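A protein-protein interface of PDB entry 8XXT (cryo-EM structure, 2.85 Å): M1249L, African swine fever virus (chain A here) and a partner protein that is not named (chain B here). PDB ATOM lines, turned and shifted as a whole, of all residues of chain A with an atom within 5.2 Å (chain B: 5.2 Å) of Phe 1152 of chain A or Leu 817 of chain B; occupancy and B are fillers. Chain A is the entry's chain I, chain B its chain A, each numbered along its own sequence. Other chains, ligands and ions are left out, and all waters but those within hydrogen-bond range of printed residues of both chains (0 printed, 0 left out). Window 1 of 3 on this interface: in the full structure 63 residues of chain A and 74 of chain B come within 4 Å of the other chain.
The side-chain hydroxyl of Ser 820 of chain B sits close to the backbone carbonyl oxygen of Pro 1151 of chain A (2.3 Å).
The side-chain hydroxyl of Ser 820 of chain B sits at hydrogen-bond distance from the backbone carbonyl oxygen of Leu 817 of chain B (3.1 Å).
The backbone carbonyl oxygen (O) of Ala 816 of chain B sits at hydrogen-bond distance from the side-chain hydroxyl (OG) of Ser 820 of chain B, at 3.1 Å.
O of Asp 1150 of chain A lies within hydrogen-bond range of OG of Ser 1153 of chain A, at 2.8 Å.
N of Phe 1152 of chain A sits close to OD1 of Asp 1150 of chain A (3.3 Å).
The backbone carbonyl oxygen (O) of Leu 817 of chain B is in hydrogen-bond range of the side-chain hydroxyl (OG) of Ser 821 of chain B (2.8 Å).
Among the printed residues, pairs that only touch across the chains: Pro 1151 of chain A with Leu 817 of chain B (3.8 Å), Phe 1152 of chain A with Ala 816 of chain B (3.6 Å), Phe 1152 of chain A with Leu 817 of chain B (3.5 Å), Phe 1152 of chain A with Ser 820 of chain B (3.3 Å) and Ser 1153 of chain A with Ser 820 of chain B (3.2 Å).
Of the printed residues of chain B, Phe 1152 of chain A touches Ala 816 (3.6 Å), Leu 817 (3.5 Å) and Ser 820 (3.3 Å).
Printed residues of chain B within 4 Å of Ser 1153 of chain A: Ser 820.
Of the printed residues of chain B, Pro 1151 of chain A touches Leu 817 and Ser 820.
Of the printed residues of chain A, Ala 816 of chain B touches Phe 1152 (3.6 Å).
Printed residues of chain A within 4 Å of Ser 820 of chain B: Pro 1151 (2.3 Å), Phe 1152 (3.3 Å) and Ser 1153 (3.2 Å).
Met 1057 of chain B touches none of the printed residues of chain A.
The nearest printed residue of chain A that does not touch Leu 817 of chain B is Asp 1150 of chain A (7.2 Å).
Hydrophobic or aromatic side chains of chain A that line the printed part of chain B: Pro 1151 and Phe 1152.
Along chain B the printed residues that touch a printed residue of chain A span positions 816 to 820.
Among the printed residues, no Asp or Glu carboxylate lies within 4 Å of a Lys or Arg side-chain nitrogen of the other chain.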
ATOM      1  N   ASP A1150      -4.664  13.760  20.537  1.00  0.00           N
ATOM      2  CA  ASP A1150      -5.727  14.283  19.688  1.00  0.00           C
ATOM      3  C   ASP A1150      -5.321  14.182  18.222  1.00  0.00           C
ATOM      4  O   ASP A1150      -4.262  14.689  17.841  1.00  0.00           O
ATOM      5  CB  ASP A1150      -6.037  15.732  20.048  1.00  0.00           C
ATOM      6  CG  ASP A1150      -7.450  16.134  19.673  1.00  0.00           C
ATOM      7  OD1 ASP A1150      -7.691  16.433  18.486  1.00  0.00           O
ATOM      8  OD2 ASP A1150      -8.320  16.148  20.567  1.00  0.00           O
ATOM      9  N   PRO A1151      -6.135  13.552  17.373  1.00  0.00           N
ATOM     10  CA  PRO A1151      -5.767  13.374  15.965  1.00  0.00           C
ATOM     11  C   PRO A1151      -5.874  14.628  15.111  1.00  0.00           C
ATOM     12  O   PRO A1151      -5.757  14.526  13.889  1.00  0.00           O
ATOM     13  CB  PRO A1151      -6.768  12.312  15.489  1.00  0.00           C
ATOM     14  CG  PRO A1151      -7.950  12.499  16.357  1.00  0.00           C
ATOM     15  CD  PRO A1151      -7.423  12.916  17.697  1.00  0.00           C
ATOM     16  N   PHE A1152      -6.102  15.795  15.707  1.00  0.00           N
ATOM     17  CA  PHE A1152      -6.171  17.041  14.960  1.00  0.00           C
ATOM     18  C   PHE A1152      -5.158  18.073  15.430  1.00  0.00           C
ATOM     19  O   PHE A1152      -5.119  19.176  14.873  1.00  0.00           O
ATOM     20  CB  PHE A1152      -7.582  17.637  15.043  1.00  0.00           C
ATOM     21  CG  PHE A1152      -8.619  16.847  14.302  1.00  0.00           C
ATOM     22  CD1 PHE A1152      -9.237  15.763  14.898  1.00  0.00           C
ATOM     23  CD2 PHE A1152      -8.975  17.187  13.012  1.00  0.00           C
ATOM     24  CE1 PHE A1152     -10.189  15.033  14.218  1.00  0.00           C
ATOM     25  CE2 PHE A1152      -9.928  16.459  12.329  1.00  0.00           C
ATOM     26  CZ  PHE A1152     -10.536  15.381  12.934  1.00  0.00           C
ATOM     27  N   SER A1153      -4.343  17.753  16.430  1.00  0.00           N
ATOM     28  CA  SER A1153      -3.380  18.712  16.949  1.00  0.00           C
ATOM     29  C   SER A1153      -2.250  18.946  15.955  1.00  0.00           C
ATOM     30  O   SER A1153      -1.967  18.115  15.089  1.00  0.00           O
ATOM     31  CB  SER A1153      -2.814  18.231  18.285  1.00  0.00           C
ATOM     32  OG  SER A1153      -2.513  16.850  18.244  1.00  0.00           O
ATOM     33  N   ILE A1154      -1.599  20.097  16.094  1.00  0.00           N
ATOM     34  CA  ILE A1154      -0.535  20.514  15.190  1.00  0.00           C
ATOM     35  C   ILE A1154       0.754  20.480  16.008  1.00  0.00           C
ATOM     36  O   ILE A1154       1.687  21.261  15.791  1.00  0.00           O
ATOM     37  CB  ILE A1154      -0.859  21.897  14.584  1.00  0.00           C
ATOM     38  CG1 ILE A1154      -2.145  21.794  13.760  1.00  0.00           C
ATOM     39  CG2 ILE A1154       0.214  22.372  13.620  1.00  0.00           C
ATOM     40  CD1 ILE A1154      -2.295  22.851  12.686  1.00  0.00           C
ATOM     41  N   ILE B 813     -13.334  16.554   6.891  1.00  0.00           N
ATOM     42  CA  ILE B 813     -12.764  15.939   8.084  1.00  0.00           C
ATOM     43  C   ILE B 813     -11.498  15.168   7.736  1.00  0.00           C
ATOM     44  O   ILE B 813     -10.506  15.215   8.472  1.00  0.00           O
ATOM     45  CB  ILE B 813     -13.807  15.035   8.761  1.00  0.00           C
ATOM     46  CG1 ILE B 813     -14.999  15.857   9.237  1.00  0.00           C
ATOM     47  CG2 ILE B 813     -13.195  14.298   9.927  1.00  0.00           C
ATOM     48  CD1 ILE B 813     -16.234  15.030   9.454  1.00  0.00           C
ATOM     49  N   ASN B 814     -11.511  14.448   6.613  1.00  0.00           N
ATOM     50  CA  ASN B 814     -10.348  13.659   6.221  1.00  0.00           C
ATOM     51  C   ASN B 814      -9.134  14.540   5.968  1.00  0.00           C
ATOM     52  O   ASN B 814      -8.007  14.166   6.311  1.00  0.00           O
ATOM     53  CB  ASN B 814     -10.671  12.833   4.980  1.00  0.00           C
ATOM     54  CG  ASN B 814     -11.542  11.645   5.290  1.00  0.00           C
ATOM     55  OD1 ASN B 814     -11.914  11.419   6.440  1.00  0.00           O
ATOM     56  ND2 ASN B 814     -11.878  10.874   4.266  1.00  0.00           N
ATOM     57  N   LYS B 815      -9.339  15.705   5.354  1.00  0.00           N
ATOM     58  CA  LYS B 815      -8.231  16.628   5.143  1.00  0.00           C
ATOM     59  C   LYS B 815      -7.602  17.049   6.462  1.00  0.00           C
ATOM     60  O   LYS B 815      -6.375  17.027   6.609  1.00  0.00           O
ATOM     61  CB  LYS B 815      -8.707  17.867   4.398  1.00  0.00           C
ATOM     62  CG  LYS B 815      -7.579  18.779   3.981  1.00  0.00           C
ATOM     63  CD  LYS B 815      -7.580  19.995   4.881  1.00  0.00           C
ATOM     64  CE  LYS B 815      -8.478  21.086   4.381  1.00  0.00           C
ATOM     65  NZ  LYS B 815      -8.571  22.167   5.398  1.00  0.00           N
ATOM     66  N   ALA B 816      -8.427  17.462   7.426  1.00  0.00           N
ATOM     67  CA  ALA B 816      -7.897  17.937   8.699  1.00  0.00           C
ATOM     68  C   ALA B 816      -7.185  16.820   9.450  1.00  0.00           C
ATOM     69  O   ALA B 816      -6.171  17.060  10.114  1.00  0.00           O
ATOM     70  CB  ALA B 816      -9.019  18.529   9.547  1.00  0.00           C
ATOM     71  N   LEU B 817      -7.704  15.594   9.362  1.00  0.00           N
ATOM     72  CA  LEU B 817      -6.994  14.455   9.931  1.00  0.00           C
ATOM     73  C   LEU B 817      -5.674  14.219   9.212  1.00  0.00           C
ATOM     74  O   LEU B 817      -4.675  13.851   9.839  1.00  0.00           O
ATOM     75  CB  LEU B 817      -7.864  13.201   9.859  1.00  0.00           C
ATOM     76  CG  LEU B 817      -8.870  12.964  10.983  1.00  0.00           C
ATOM     77  CD1 LEU B 817     -10.142  12.350  10.432  1.00  0.00           C
ATOM     78  CD2 LEU B 817      -8.269  12.072  12.050  1.00  0.00           C
ATOM     79  N   SER B 818      -5.649  14.428   7.895  1.00  0.00           N
ATOM     80  CA  SER B 818      -4.461  14.104   7.112  1.00  0.00           C
ATOM     81  C   SER B 818      -3.260  14.932   7.548  1.00  0.00           C
ATOM     82  O   SER B 818      -2.143  14.413   7.644  1.00  0.00           O
ATOM     83  CB  SER B 818      -4.736  14.318   5.626  1.00  0.00           C
ATOM     84  OG  SER B 818      -4.530  15.673   5.269  1.00  0.00           O
ATOM     85  N   THR B 819      -3.463  16.226   7.803  1.00  0.00           N
ATOM     86  CA  THR B 819      -2.351  17.078   8.213  1.00  0.00           C
ATOM     87  C   THR B 819      -1.772  16.624   9.547  1.00  0.00           C
ATOM     88  O   THR B 819      -0.552  16.493   9.697  1.00  0.00           O
ATOM     89  CB  THR B 819      -2.811  18.535   8.295  1.00  0.00           C
ATOM     90  OG1 THR B 819      -2.800  19.116   6.985  1.00  0.00           O
ATOM     91  CG2 THR B 819      -1.893  19.340   9.205  1.00  0.00           C
ATOM     92  N   SER B 820      -2.636  16.365  10.527  1.00  0.00           N
ATOM     93  CA  SER B 820      -2.161  16.002  11.856  1.00  0.00           C
ATOM     94  C   SER B 820      -1.650  14.569  11.910  1.00  0.00           C
ATOM     95  O   SER B 820      -0.638  14.295  12.564  1.00  0.00           O
ATOM     96  CB  SER B 820      -3.276  16.201  12.878  1.00  0.00           C
ATOM     97  OG  SER B 820      -4.504  15.691  12.390  1.00  0.00           O
ATOM     98  N   SER B 821      -2.343  13.639  11.250  1.00  0.00           N
ATOM     99  CA  SER B 821      -1.940  12.239  11.312  1.00  0.00           C
ATOM    100  C   SER B 821      -0.576  12.027  10.674  1.00  0.00           C
ATOM    101  O   SER B 821       0.260  11.292  11.210  1.00  0.00           O
ATOM    102  CB  SER B 821      -2.990  11.357  10.639  1.00  0.00           C
ATOM    103  OG  SER B 821      -4.250  11.500  11.270  1.00  0.00           O
ATOM    104  N   THR B 822      -0.331  12.660   9.528  1.00  0.00           N
ATOM    105  CA  THR B 822       0.966  12.526   8.883  1.00  0.00           C
ATOM    106  C   THR B 822       2.055  13.301   9.609  1.00  0.00           C
ATOM    107  O   THR B 822       3.234  12.963   9.469  1.00  0.00           O
ATOM    108  CB  THR B 822       0.886  12.984   7.428  1.00  0.00           C
ATOM    109  OG1 THR B 822       0.494  14.360   7.380  1.00  0.00           O
ATOM    110  CG2 THR B 822      -0.128  12.149   6.675  1.00  0.00           C
ATOM    111  N   MET B1057      -4.758   9.168   3.553  1.00  0.00           N
ATOM    112  CA  MET B1057      -5.897   9.542   4.384  1.00  0.00           C
ATOM    113  C   MET B1057      -7.054  10.025   3.525  1.00  0.00           C
ATOM    114  O   MET B1057      -8.216   9.694   3.787  1.00  0.00           O
ATOM    115  CB  MET B1057      -5.484  10.634   5.365  1.00  0.00           C
ATOM    116  CG  MET B1057      -4.286  10.235   6.164  1.00  0.00           C
ATOM    117  SD  MET B1057      -4.164   8.446   6.206  1.00  0.00           S
ATOM    118  CE  MET B1057      -2.736   8.278   7.246  1.00  0.00           C
